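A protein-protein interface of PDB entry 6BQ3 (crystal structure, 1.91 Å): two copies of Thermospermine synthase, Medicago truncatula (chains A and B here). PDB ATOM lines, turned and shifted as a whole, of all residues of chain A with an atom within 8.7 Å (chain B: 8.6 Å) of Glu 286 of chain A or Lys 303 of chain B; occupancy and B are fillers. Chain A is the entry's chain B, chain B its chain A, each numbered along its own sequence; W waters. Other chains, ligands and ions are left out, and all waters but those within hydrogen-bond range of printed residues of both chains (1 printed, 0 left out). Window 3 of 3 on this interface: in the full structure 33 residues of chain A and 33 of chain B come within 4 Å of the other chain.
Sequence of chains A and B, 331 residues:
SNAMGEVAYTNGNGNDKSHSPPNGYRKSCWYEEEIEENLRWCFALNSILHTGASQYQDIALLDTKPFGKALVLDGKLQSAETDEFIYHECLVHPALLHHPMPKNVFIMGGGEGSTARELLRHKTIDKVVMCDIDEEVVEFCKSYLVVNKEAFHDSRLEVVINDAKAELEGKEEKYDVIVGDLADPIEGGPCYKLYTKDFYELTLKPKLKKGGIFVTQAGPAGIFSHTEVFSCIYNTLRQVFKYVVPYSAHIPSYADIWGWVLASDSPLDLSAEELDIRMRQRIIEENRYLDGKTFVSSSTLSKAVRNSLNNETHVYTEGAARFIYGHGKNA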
ATOM      1  N   PHE A  85      14.278 -19.940  18.423  1.00  0.00           N
ATOM      2  CA  PHE A  85      14.154 -21.289  17.860  1.00  0.00           C
ATOM      3  C   PHE A  85      15.420 -22.144  17.936  1.00  0.00           C
ATOM      4  O   PHE A  85      15.348 -23.340  18.197  1.00  0.00           O
ATOM      5  CB  PHE A  85      13.586 -21.293  16.431  1.00  0.00           C
ATOM      6  CG  PHE A  85      14.541 -20.908  15.327  1.00  0.00           C
ATOM      7  CD1 PHE A  85      15.243 -21.855  14.618  1.00  0.00           C
ATOM      8  CD2 PHE A  85      14.631 -19.595  14.904  1.00  0.00           C
ATOM      9  CE1 PHE A  85      16.083 -21.491  13.583  1.00  0.00           C
ATOM     10  CE2 PHE A  85      15.436 -19.234  13.828  1.00  0.00           C
ATOM     11  CZ  PHE A  85      16.176 -20.187  13.178  1.00  0.00           C
ATOM     12  N   GLU A  89      15.243 -25.427  20.027  1.00  0.00           N
ATOM     13  CA  GLU A  89      15.445 -26.656  19.260  1.00  0.00           C
ATOM     14  C   GLU A  89      16.633 -27.420  19.776  1.00  0.00           C
ATOM     15  O   GLU A  89      16.534 -28.646  19.926  1.00  0.00           O
ATOM     16  CB  GLU A  89      15.544 -26.469  17.748  1.00  0.00           C
ATOM     17  CG  GLU A  89      14.253 -26.041  17.079  1.00  0.00           C
ATOM     18  CD  GLU A  89      14.343 -26.009  15.571  1.00  0.00           C
ATOM     19  OE1 GLU A  89      15.322 -26.510  15.032  1.00  0.00           O
ATOM     20  OE2 GLU A  89      13.414 -25.512  14.919  1.00  0.00           O
ATOM     21  N   HIS A  93      15.332 -31.024  21.302  1.00  0.00           N
ATOM     22  CA  HIS A  93      15.157 -32.174  20.392  1.00  0.00           C
ATOM     23  C   HIS A  93      16.209 -33.282  20.563  1.00  0.00           C
ATOM     24  O   HIS A  93      15.857 -34.447  20.516  1.00  0.00           O
ATOM     25  CB  HIS A  93      14.980 -31.711  18.981  1.00  0.00           C
ATOM     26  CG  HIS A  93      13.758 -30.869  18.819  1.00  0.00           C
ATOM     27  ND1 HIS A  93      12.540 -31.264  19.323  1.00  0.00           N
ATOM     28  CD2 HIS A  93      13.584 -29.641  18.312  1.00  0.00           C
ATOM     29  CE1 HIS A  93      11.653 -30.317  19.085  1.00  0.00           C
ATOM     30  NE2 HIS A  93      12.260 -29.327  18.454  1.00  0.00           N
ATOM     31  N   GLU A 118       8.448 -26.676  21.977  1.00  0.00           N
ATOM     32  CA  GLU A 118       9.178 -27.640  21.186  1.00  0.00           C
ATOM     33  C   GLU A 118       8.969 -29.070  21.710  1.00  0.00           C
ATOM     34  O   GLU A 118       8.923 -29.983  20.916  1.00  0.00           O
ATOM     35  CB  GLU A 118      10.651 -27.283  21.192  1.00  0.00           C
ATOM     36  CG  GLU A 118      10.931 -25.936  20.521  1.00  0.00           C
ATOM     37  CD  GLU A 118      10.613 -25.951  19.040  1.00  0.00           C
ATOM     38  OE1 GLU A 118      10.819 -27.004  18.382  1.00  0.00           O
ATOM     39  OE2 GLU A 118      10.152 -24.930  18.535  1.00  0.00           O
ATOM     40  N   ARG A 121       5.674 -30.461  20.209  1.00  0.00           N
ATOM     41  CA  ARG A 121       5.779 -30.920  18.837  1.00  0.00           C
ATOM     42  C   ARG A 121       6.071 -32.406  18.726  1.00  0.00           C
ATOM     43  O   ARG A 121       5.906 -32.996  17.648  1.00  0.00           O
ATOM     44  CB  ARG A 121       6.845 -30.126  18.107  1.00  0.00           C
ATOM     45  CG  ARG A 121       6.551 -28.631  17.946  1.00  0.00           C
ATOM     46  CD  ARG A 121       7.677 -27.898  17.211  1.00  0.00           C
ATOM     47  NE  ARG A 121       7.940 -28.474  15.892  1.00  0.00           N
ATOM     48  CZ  ARG A 121       9.141 -28.514  15.294  1.00  0.00           C
ATOM     49  NH1 ARG A 121      10.221 -28.018  15.910  1.00  0.00           N
ATOM     50  NH2 ARG A 121       9.276 -29.114  14.105  1.00  0.00           N
ATOM     51  N   ASP A 276      17.533 -37.985  11.884  1.00  0.00           N
ATOM     52  CA  ASP A 276      16.578 -37.491  10.893  1.00  0.00           C
ATOM     53  C   ASP A 276      15.325 -38.354  10.783  1.00  0.00           C
ATOM     54  O   ASP A 276      14.226 -37.827  10.658  1.00  0.00           O
ATOM     55  CB  ASP A 276      17.256 -37.335   9.528  1.00  0.00           C
ATOM     56  CG  ASP A 276      18.201 -36.160   9.477  1.00  0.00           C
ATOM     57  OD1 ASP A 276      18.035 -35.218  10.272  1.00  0.00           O
ATOM     58  OD2 ASP A 276      19.119 -36.159   8.655  1.00  0.00           O
ATOM     59  N   MET A 279      13.215 -37.640  13.738  1.00  0.00           N
ATOM     60  CA  MET A 279      12.567 -36.342  13.527  1.00  0.00           C
ATOM     61  C   MET A 279      11.339 -36.474  12.653  1.00  0.00           C
ATOM     62  O   MET A 279      10.244 -36.018  12.987  1.00  0.00           O
ATOM     63  CB  MET A 279      13.554 -35.311  12.949  1.00  0.00           C
ATOM     64  CG  MET A 279      14.633 -34.930  13.962  1.00  0.00           C
ATOM     65  SD  MET A 279      15.707 -33.658  13.325  1.00  0.00           S
ATOM     66  CE  MET A 279      17.185 -34.008  14.285  1.00  0.00           C
ATOM     67  N   ARG A 280      11.529 -37.156  11.541  1.00  0.00           N
ATOM     68  CA  ARG A 280      10.460 -37.361  10.603  1.00  0.00           C
ATOM     69  C   ARG A 280       9.300 -38.160  11.197  1.00  0.00           C
ATOM     70  O   ARG A 280       8.140 -37.844  10.916  1.00  0.00           O
ATOM     71  CB  ARG A 280      10.995 -38.054   9.335  1.00  0.00           C
ATOM     72  CG  ARG A 280       9.974 -38.192   8.210  1.00  0.00           C
ATOM     73  CD  ARG A 280       9.537 -36.820   7.696  1.00  0.00           C
ATOM     74  NE  ARG A 280      10.462 -36.318   6.673  1.00  0.00           N
ATOM     75  CZ  ARG A 280      10.414 -36.660   5.376  1.00  0.00           C
ATOM     76  NH1 ARG A 280       9.464 -37.493   4.934  1.00  0.00           N
ATOM     77  NH2 ARG A 280      11.293 -36.157   4.527  1.00  0.00           N
ATOM     78  N   ILE A 283       8.167 -35.820  15.176  1.00  0.00           N
ATOM     79  CA  ILE A 283       8.028 -34.372  15.389  1.00  0.00           C
ATOM     80  C   ILE A 283       7.105 -33.785  14.367  1.00  0.00           C
ATOM     81  O   ILE A 283       7.317 -33.956  13.178  1.00  0.00           O
ATOM     82  CB  ILE A 283       9.366 -33.618  15.357  1.00  0.00           C
ATOM     83  CG1 ILE A 283      10.312 -34.223  16.361  1.00  0.00           C
ATOM     84  CG2 ILE A 283       9.152 -32.140  15.706  1.00  0.00           C
ATOM     85  CD1 ILE A 283      11.656 -33.535  16.431  1.00  0.00           C
ATOM     86  N   ILE A 284       6.097 -33.075  14.834  1.00  0.00           N
ATOM     87  CA  ILE A 284       5.176 -32.380  13.944  1.00  0.00           C
ATOM     88  C   ILE A 284       5.935 -31.178  13.354  1.00  0.00           C
ATOM     89  O   ILE A 284       6.638 -30.487  14.093  1.00  0.00           O
ATOM     90  CB  ILE A 284       3.936 -31.906  14.716  1.00  0.00           C
ATOM     91  CG1 ILE A 284       3.170 -33.113  15.302  1.00  0.00           C
ATOM     92  CG2 ILE A 284       3.031 -31.112  13.797  1.00  0.00           C
ATOM     93  CD1 ILE A 284       2.209 -32.760  16.425  1.00  0.00           C
ATOM     94  N   GLU A 285       5.819 -31.002  12.042  1.00  0.00           N
ATOM     95  CA  GLU A 285       6.454 -29.940  11.241  1.00  0.00           C
ATOM     96  C   GLU A 285       7.949 -30.073  11.127  1.00  0.00           C
ATOM     97  O   GLU A 285       8.567 -30.887  11.800  1.00  0.00           O
ATOM     98  CB  GLU A 285       6.121 -28.535  11.763  1.00  0.00           C
ATOM     99  CG  GLU A 285       4.646 -28.221  11.787  1.00  0.00           C
ATOM    100  CD  GLU A 285       4.333 -26.838  12.341  1.00  0.00           C
ATOM    101  OE1 GLU A 285       3.326 -26.709  13.082  1.00  0.00           O
ATOM    102  OE2 GLU A 285       5.071 -25.870  12.014  1.00  0.00           O
ATOM    103  N   GLU A 286       8.534 -29.224  10.293  1.00  0.00           N
ATOM    104  CA  GLU A 286       9.973 -29.213  10.078  1.00  0.00           C
ATOM    105  C   GLU A 286      10.678 -28.340  11.106  1.00  0.00           C
ATOM    106  O   GLU A 286      10.283 -27.200  11.315  1.00  0.00           O
ATOM    107  CB  GLU A 286      10.293 -28.644   8.688  1.00  0.00           C
ATOM    108  CG  GLU A 286       9.935 -29.564   7.517  1.00  0.00           C
ATOM    109  CD  GLU A 286      11.102 -30.451   7.106  1.00  0.00           C
ATOM    110  OE1 GLU A 286      12.217 -29.903   6.791  1.00  0.00           O
ATOM    111  OE2 GLU A 286      10.923 -31.686   7.110  1.00  0.00           O
ATOM    112  N   ASN A 287      11.753 -28.875  11.685  1.00  0.00           N
ATOM    113  CA  ASN A 287      12.725 -28.093  12.457  1.00  0.00           C
ATOM    114  C   ASN A 287      13.333 -27.060  11.530  1.00  0.00           C
ATOM    115  O   ASN A 287      13.524 -27.319  10.320  1.00  0.00           O
ATOM    116  CB  ASN A 287      13.814 -29.007  13.028  1.00  0.00           C
ATOM    117  CG  ASN A 287      13.333 -29.844  14.190  1.00  0.00           C
ATOM    118  OD1 ASN A 287      12.219 -29.663  14.683  1.00  0.00           O
ATOM    119  ND2 ASN A 287      14.197 -30.722  14.692  1.00  0.00           N
ATOM    120  N   ARG A 288      13.537 -25.862  12.056  1.00  0.00           N
ATOM    121  CA  ARG A 288      14.115 -24.781  11.306  1.00  0.00           C
ATOM    122  C   ARG A 288      15.633 -24.749  11.501  1.00  0.00           C
ATOM    123  O   ARG A 288      16.349 -24.277  10.616  1.00  0.00           O
ATOM    124  CB  ARG A 288      13.472 -23.461  11.723  1.00  0.00           C
ATOM    125  CG  ARG A 288      11.929 -23.497  11.656  1.00  0.00           C
ATOM    126  CD  ARG A 288      11.328 -22.386  12.493  1.00  0.00           C
ATOM    127  NE  ARG A 288      11.797 -21.095  11.981  1.00  0.00           N
ATOM    128  CZ  ARG A 288      11.876 -19.976  12.710  1.00  0.00           C
ATOM    129  NH1 ARG A 288      12.314 -18.851  12.154  1.00  0.00           N
ATOM    130  NH2 ARG A 288      11.499 -19.980  13.990  1.00  0.00           N
ATOM    131  N   TYR A 289      16.134 -25.255  12.641  1.00  0.00           N
ATOM    132  CA  TYR A 289      17.563 -25.186  12.912  1.00  0.00           C
ATOM    133  C   TYR A 289      18.218 -26.535  12.844  1.00  0.00           C
ATOM    134  O   TYR A 289      19.258 -26.682  12.263  1.00  0.00           O
ATOM    135  CB  TYR A 289      17.886 -24.596  14.275  1.00  0.00           C
ATOM    136  CG  TYR A 289      19.352 -24.527  14.469  1.00  0.00           C
ATOM    137  CD1 TYR A 289      20.100 -23.580  13.809  1.00  0.00           C
ATOM    138  CD2 TYR A 289      20.008 -25.466  15.248  1.00  0.00           C
ATOM    139  CE1 TYR A 289      21.466 -23.539  13.958  1.00  0.00           C
ATOM    140  CE2 TYR A 289      21.383 -25.417  15.414  1.00  0.00           C
ATOM    141  CZ  TYR A 289      22.083 -24.491  14.759  1.00  0.00           C
ATOM    142  OH  TYR A 289      23.423 -24.509  14.932  1.00  0.00           O
ATOM    143  N   LEU A 290      17.627 -27.512  13.493  1.00  0.00           N
ATOM    144  CA  LEU A 290      18.302 -28.761  13.788  1.00  0.00           C
ATOM    145  C   LEU A 290      17.898 -29.893  12.868  1.00  0.00           C
ATOM    146  O   LEU A 290      16.729 -30.265  12.846  1.00  0.00           O
ATOM    147  CB  LEU A 290      17.957 -29.144  15.214  1.00  0.00           C
ATOM    148  CG  LEU A 290      18.914 -30.141  15.843  1.00  0.00           C
ATOM    149  CD1 LEU A 290      20.234 -29.528  16.190  1.00  0.00           C
ATOM    150  CD2 LEU A 290      18.297 -30.730  17.084  1.00  0.00           C
ATOM    151  N   ASP A 291      18.852 -30.406  12.086  1.00  0.00           N
ATOM    152  CA  ASP A 291      18.753 -31.766  11.529  1.00  0.00           C
ATOM    153  C   ASP A 291      19.834 -32.645  12.174  1.00  0.00           C
ATOM    154  O   ASP A 291      20.574 -32.220  13.076  1.00  0.00           O
ATOM    155  CB  ASP A 291      18.765 -31.789   9.984  1.00  0.00           C
ATOM    156  CG  ASP A 291      20.034 -31.191   9.362  1.00  0.00           C
ATOM    157  OD1 ASP A 291      21.017 -30.894  10.081  1.00  0.00           O
ATOM    158  OD2 ASP A 291      20.066 -31.042   8.158  1.00  0.00           O
ATOM    159  N   GLY A 292      19.891 -33.896  11.753  1.00  0.00           N
ATOM    160  CA  GLY A 292      20.893 -34.841  12.252  1.00  0.00           C
ATOM    161  C   GLY A 292      22.316 -34.362  12.071  1.00  0.00           C
ATOM    162  O   GLY A 292      23.126 -34.417  13.012  1.00  0.00           O
ATOM    163  N   LYS A 293      22.645 -33.843  10.886  1.00  0.00           N
ATOM    164  CA  LYS A 293      24.034 -33.381  10.659  1.00  0.00           C
ATOM    165  C   LYS A 293      24.369 -32.235  11.624  1.00  0.00           C
ATOM    166  O   LYS A 293      25.489 -32.143  12.152  1.00  0.00           O
ATOM    167  CB  LYS A 293      24.285 -32.955   9.199  1.00  0.00           C
ATOM    168  CG  LYS A 293      24.366 -34.069   8.137  1.00  0.00           C
ATOM    169  CD  LYS A 293      24.874 -33.465   6.806  1.00  0.00           C
ATOM    170  CE  LYS A 293      25.217 -34.468   5.727  1.00  0.00           C
ATOM    171  NZ  LYS A 293      25.902 -33.836   4.543  1.00  0.00           N
ATOM    172  N   THR A 294      23.391 -31.340  11.833  1.00  0.00           N
ATOM    173  CA  THR A 294      23.614 -30.151  12.604  1.00  0.00           C
ATOM    174  C   THR A 294      23.946 -30.603  14.020  1.00  0.00           C
ATOM    175  O   THR A 294      24.815 -30.023  14.641  1.00  0.00           O
ATOM    176  CB  THR A 294      22.411 -29.175  12.582  1.00  0.00           C
ATOM    177  OG1 THR A 294      22.121 -28.761  11.232  1.00  0.00           O
ATOM    178  CG2 THR A 294      22.681 -27.907  13.473  1.00  0.00           C
ATOM    179  N   PHE A 295      23.224 -31.589  14.538  1.00  0.00           N
ATOM    180  CA  PHE A 295      23.508 -32.107  15.863  1.00  0.00           C
ATOM    181  C   PHE A 295      24.922 -32.717  15.941  1.00  0.00           C
ATOM    182  O   PHE A 295      25.663 -32.427  16.894  1.00  0.00           O
ATOM    183  CB  PHE A 295      22.485 -33.128  16.395  1.00  0.00           C
ATOM    184  CG  PHE A 295      22.848 -33.602  17.767  1.00  0.00           C
ATOM    185  CD1 PHE A 295      22.776 -32.720  18.858  1.00  0.00           C
ATOM    186  CD2 PHE A 295      23.395 -34.848  17.970  1.00  0.00           C
ATOM    187  CE1 PHE A 295      23.220 -33.105  20.112  1.00  0.00           C
ATOM    188  CE2 PHE A 295      23.836 -35.230  19.227  1.00  0.00           C
ATOM    189  CZ  PHE A 295      23.724 -34.372  20.286  1.00  0.00           C
ATOM    190  N   SER A 297      27.531 -31.981  14.156  1.00  0.00           N
ATOM    191  CA  SER A 297      28.429 -30.857  14.115  1.00  0.00           C
ATOM    192  C   SER A 297      28.486 -30.152  15.493  1.00  0.00           C
ATOM    193  O   SER A 297      29.569 -29.840  16.024  1.00  0.00           O
ATOM    194  CB  SER A 297      27.984 -29.875  13.030  1.00  0.00           C
ATOM    195  OG  SER A 297      28.831 -28.705  12.952  1.00  0.00           O
ATOM    196  N   ILE B 223      23.663 -17.625  11.075  1.00  0.00           N
ATOM    197  CA  ILE B 223      22.331 -18.078  10.667  1.00  0.00           C
ATOM    198  C   ILE B 223      21.599 -17.115   9.743  1.00  0.00           C
ATOM    199  O   ILE B 223      21.097 -17.556   8.722  1.00  0.00           O
ATOM    200  CB  ILE B 223      21.495 -18.481  11.915  1.00  0.00           C
ATOM    201  CG1 ILE B 223      20.110 -19.047  11.549  1.00  0.00           C
ATOM    202  CG2 ILE B 223      21.269 -17.328  12.878  1.00  0.00           C
ATOM    203  CD1 ILE B 223      20.183 -20.287  10.707  1.00  0.00           C
ATOM    204  N   HIS B 226      24.918 -14.781   7.111  1.00  0.00           N
ATOM    205  CA  HIS B 226      25.535 -15.457   5.979  1.00  0.00           C
ATOM    206  C   HIS B 226      24.989 -15.091   4.570  1.00  0.00           C
ATOM    207  O   HIS B 226      25.656 -15.350   3.580  1.00  0.00           O
ATOM    208  CB  HIS B 226      25.407 -16.959   6.127  1.00  0.00           C
ATOM    209  CG  HIS B 226      24.064 -17.490   5.728  1.00  0.00           C
ATOM    210  ND1 HIS B 226      23.013 -17.629   6.605  1.00  0.00           N
ATOM    211  CD2 HIS B 226      23.600 -17.893   4.518  1.00  0.00           C
ATOM    212  CE1 HIS B 226      21.967 -18.128   5.958  1.00  0.00           C
ATOM    213  NE2 HIS B 226      22.298 -18.299   4.693  1.00  0.00           N
ATOM    214  N   THR B 300      30.409 -28.798   8.191  1.00  0.00           N
ATOM    215  CA  THR B 300      29.032 -29.305   8.379  1.00  0.00           C
ATOM    216  C   THR B 300      28.244 -28.122   8.838  1.00  0.00           C
ATOM    217  O   THR B 300      28.159 -27.853   9.997  1.00  0.00           O
ATOM    218  CB  THR B 300      28.960 -30.411   9.439  1.00  0.00           C
ATOM    219  OG1 THR B 300      29.957 -31.383   9.148  1.00  0.00           O
ATOM    220  CG2 THR B 300      27.579 -31.106   9.424  1.00  0.00           C
ATOM    221  N   LEU B 301      27.707 -27.384   7.882  1.00  0.00           N
ATOM    222  CA  LEU B 301      26.961 -26.183   8.153  1.00  0.00           C
ATOM    223  C   LEU B 301      25.625 -26.580   8.759  1.00  0.00           C
ATOM    224  O   LEU B 301      25.253 -27.751   8.695  1.00  0.00           O
ATOM    225  CB  LEU B 301      26.777 -25.402   6.854  1.00  0.00           C
ATOM    226  CG  LEU B 301      28.127 -24.987   6.252  1.00  0.00           C
ATOM    227  CD1 LEU B 301      27.981 -24.360   4.875  1.00  0.00           C
ATOM    228  CD2 LEU B 301      28.891 -24.102   7.220  1.00  0.00           C
ATOM    229  N   SER B 302      24.900 -25.636   9.330  1.00  0.00           N
ATOM    230  CA  SER B 302      23.605 -26.000   9.914  1.00  0.00           C
ATOM    231  C   SER B 302      22.560 -26.186   8.821  1.00  0.00           C
ATOM    232  O   SER B 302      22.743 -25.711   7.684  1.00  0.00           O
ATOM    233  CB  SER B 302      23.147 -24.963  10.898  1.00  0.00           C
ATOM    234  OG  SER B 302      22.666 -23.822  10.221  1.00  0.00           O
ATOM    235  N   LYS B 303      21.456 -26.854   9.166  1.00  0.00           N
ATOM    236  CA  LYS B 303      20.377 -27.098   8.212  1.00  0.00           C
ATOM    237  C   LYS B 303      20.052 -25.873   7.355  1.00  0.00           C
ATOM    238  O   LYS B 303      20.082 -25.919   6.106  1.00  0.00           O
ATOM    239  CB  LYS B 303      19.101 -27.535   8.957  1.00  0.00           C
ATOM    240  CG  LYS B 303      18.013 -28.033   8.020  1.00  0.00           C
ATOM    241  CD  LYS B 303      16.775 -28.445   8.784  1.00  0.00           C
ATOM    242  CE  LYS B 303      15.634 -28.622   7.803  1.00  0.00           C
ATOM    243  NZ  LYS B 303      14.451 -29.222   8.443  1.00  0.00           N
ATOM    244  N   ALA B 304      19.737 -24.778   8.030  1.00  0.00           N
ATOM    245  CA  ALA B 304      19.269 -23.590   7.338  1.00  0.00           C
ATOM    246  C   ALA B 304      20.382 -22.961   6.462  1.00  0.00           C
ATOM    247  O   ALA B 304      20.120 -22.582   5.331  1.00  0.00           O
ATOM    248  CB  ALA B 304      18.712 -22.588   8.325  1.00  0.00           C
ATOM    249  N   VAL B 305      21.611 -22.881   6.974  1.00  0.00           N
ATOM    250  CA  VAL B 305      22.700 -22.310   6.203  1.00  0.00           C
ATOM    251  C   VAL B 305      23.001 -23.150   4.965  1.00  0.00           C
ATOM    252  O   VAL B 305      23.077 -22.612   3.859  1.00  0.00           O
ATOM    253  CB  VAL B 305      23.952 -22.072   7.077  1.00  0.00           C
ATOM    254  CG1 VAL B 305      25.145 -21.628   6.221  1.00  0.00           C
ATOM    255  CG2 VAL B 305      23.655 -21.011   8.102  1.00  0.00           C
ATOM    256  N   ARG B 306      23.095 -24.466   5.153  1.00  0.00           N
ATOM    257  CA  ARG B 306      23.343 -25.411   4.097  1.00  0.00           C
ATOM    258  C   ARG B 306      22.289 -25.300   2.953  1.00  0.00           C
ATOM    259  O   ARG B 306      22.632 -25.345   1.757  1.00  0.00           O
ATOM    260  CB  ARG B 306      23.334 -26.835   4.691  1.00  0.00           C
ATOM    261  CG  ARG B 306      24.363 -27.794   4.149  1.00  0.00           C
ATOM    262  CD  ARG B 306      24.138 -29.212   4.652  1.00  0.00           C
ATOM    263  NE  ARG B 306      24.138 -29.291   6.103  1.00  0.00           N
ATOM    264  CZ  ARG B 306      23.139 -29.813   6.847  1.00  0.00           C
ATOM    265  NH1 ARG B 306      22.045 -30.317   6.258  1.00  0.00           N
ATOM    266  NH2 ARG B 306      23.223 -29.795   8.201  1.00  0.00           N
ATOM    267  N   ASN B 307      21.019 -25.147   3.327  1.00  0.00           N
ATOM    268  CA  ASN B 307      19.926 -25.008   2.358  1.00  0.00           C
ATOM    269  C   ASN B 307      19.914 -23.633   1.702  1.00  0.00           C
ATOM    270  O   ASN B 307      19.661 -23.505   0.517  1.00  0.00           O
ATOM    271  CB  ASN B 307      18.573 -25.281   3.010  1.00  0.00           C
ATOM    272  CG  ASN B 307      18.385 -26.746   3.358  1.00  0.00           C
ATOM    273  OD1 ASN B 307      19.101 -27.597   2.850  1.00  0.00           O
ATOM    274  ND2 ASN B 307      17.392 -27.047   4.169  1.00  0.00           N
ATOM    275  N   SER B 308      20.197 -22.610   2.477  1.00  0.00           N
ATOM    276  CA  SER B 308      20.349 -21.260   1.955  1.00  0.00           C
ATOM    277  C   SER B 308      21.470 -21.180   0.880  1.00  0.00           C
ATOM    278  O   SER B 308      21.240 -20.711  -0.266  1.00  0.00           O
ATOM    279  CB  SER B 308      20.580 -20.328   3.133  1.00  0.00           C
ATOM    280  OG  SER B 308      20.640 -18.987   2.749  1.00  0.00           O
ATOM    281  N   LEU B 309      22.640 -21.714   1.205  1.00  0.00           N
ATOM    282  CA  LEU B 309      23.760 -21.735   0.245  1.00  0.00           C
ATOM    283  C   LEU B 309      23.412 -22.459  -1.065  1.00  0.00           C
ATOM    284  O   LEU B 309      23.710 -21.971  -2.176  1.00  0.00           O
ATOM    285  CB  LEU B 309      25.011 -22.380   0.858  1.00  0.00           C
ATOM    286  CG  LEU B 309      26.037 -21.379   1.407  1.00  0.00           C
ATOM    287  CD1 LEU B 309      25.437 -20.407   2.412  1.00  0.00           C
ATOM    288  CD2 LEU B 309      27.218 -22.133   2.015  1.00  0.00           C
ATOM    289  N   ASN B 310      22.796 -23.618  -0.909  1.00  0.00           N
ATOM    290  CA  ASN B 310      22.404 -24.447  -2.029  1.00  0.00           C
ATOM    291  C   ASN B 310      21.437 -23.715  -2.987  1.00  0.00           C
ATOM    292  O   ASN B 310      21.593 -23.776  -4.209  1.00  0.00           O
ATOM    293  CB  ASN B 310      21.779 -25.741  -1.523  1.00  0.00           C
ATOM    294  CG  ASN B 310      21.294 -26.601  -2.636  1.00  0.00           C
ATOM    295  OD1 ASN B 310      20.100 -26.866  -2.758  1.00  0.00           O
ATOM    296  ND2 ASN B 310      22.208 -26.997  -3.505  1.00  0.00           N
HETATM  297  O   HOH W   1      20.025 -24.305  10.821  1.00  0.00           O
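ND2 of Asn 287 of chain A is in hydrogen-bond range of O of Leu 290 of chain A, 3.2 Å away. The side-chain carboxylate (OD1) of Asp 291 of chain A lies close to the backbone NH (N) of Lys 293 of chain A, 3.5 Å away. The side-chain sulfur (SD) of Met 279 of chain A sits at hydrogen-bond distance from the side-chain amide nitrogen (ND2) of Asn 287 of chain A (3.6 Å).
Among the printed residues, pairs that only touch across the chains: Arg 288 of chain A with Ala 304 of chain B, Tyr 289 of chain A with Ser 302 of chain B, Tyr 289 of chain A with Lys 303 of chain B, Asp 291 of chain A with Lys 303 of chain B, Lys 293 of chain A with Thr 300 of chain B, Lys 293 of chain A with Arg 306 of chain B and Thr 294 of chain A with Ser 302 of chain B.
OG1 of Thr 294 of chain A lies within hydrogen-bond range of NH2 of Arg 306 of chain B (3.4 Å). The side-chain amino group (NZ) of Lys 303 of chain B sits at hydrogen-bond distance from the backbone carbonyl oxygen (O) of Asn 287 of chain A (2.8 Å). The side-chain carboxylate (OE1) of Glu 286 of chain A lies within salt-bridge range of the side-chain amino group (NZ) of Lys 303 of chain B, 2.9 Å away. NH1 of Arg 306 of chain B lies within salt-bridge range of OD2 of Asp 291 of chain A. The side-chain hydroxyl (OG1) of Thr 294 of chain A lies within hydrogen-bond range of the backbone NH (N) of Lys 303 of chain B. The side-chain hydroxyl (OG) of Ser 297 of chain A lies within hydrogen-bond range of the backbone carbonyl oxygen (O) of Thr 300 of chain B, at 3.1 Å.
Of the printed residues of chain B, Tyr 289 of chain A touches Ser 302 (3.8 Å) and Lys 303 (3.4 Å). Of the printed residues of chain B, Lys 293 of chain A touches Thr 300 (3.6 Å) and Arg 306 (3.5 Å). Of the printed residues of chain A, Thr 300 of chain B touches Lys 293 and Ser 297. Of chain A, only Tyr 289 and Thr 294 come within 4 Å of Ser 302 of chain B. Lys 303 of chain B touches just these residues of chain A: Glu 286, Asn 287, Tyr 289, Asp 291 and Thr 294. The nearest residue of chain B that does not touch Glu 286 of chain A is Asn 307 of chain B (6.5 Å). The nearest residue of chain A that does not touch Lys 303 of chain B is Leu 290 of chain A (4.5 Å).
Of the 13 printed residues of chain B, 5 touch a printed residue of chain A. Printed residues of chain B that touch a printed residue of chain A: Thr 300, Ser 302, Lys 303, Ala 304 and Arg 306. Hydrophobic or aromatic side chains of chain B within 4 Å of the printed part of chain A: Ala 304. Along chain B the printed residues that touch a printed residue of chain A span positions 300 to 306. Among the printed residues, Asp or Glu carboxylates within 4 Å of a Lys or Arg side-chain nitrogen of the other chain: Glu 286 of chain A with Lys 303 of chain B and Asp 291 of chain A with Arg 306 of chain B.
No position is printed for both chains. Of the 13 pairs that touch across the chains among the printed residues, none has its exchanged pair printed and touching as well.
Water W1 lies within hydrogen-bond range of the side-chain hydroxyl (OG) of Ser 302 of chain B (2.8 Å), the backbone NH (N) of Ala 304 of chain B (2.8 Å), the backbone carbonyl oxygen (O) of Tyr 289 of chain A (2.9 Å) and the backbone NH (N) of Lys 303 of chain B (3.4 Å).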
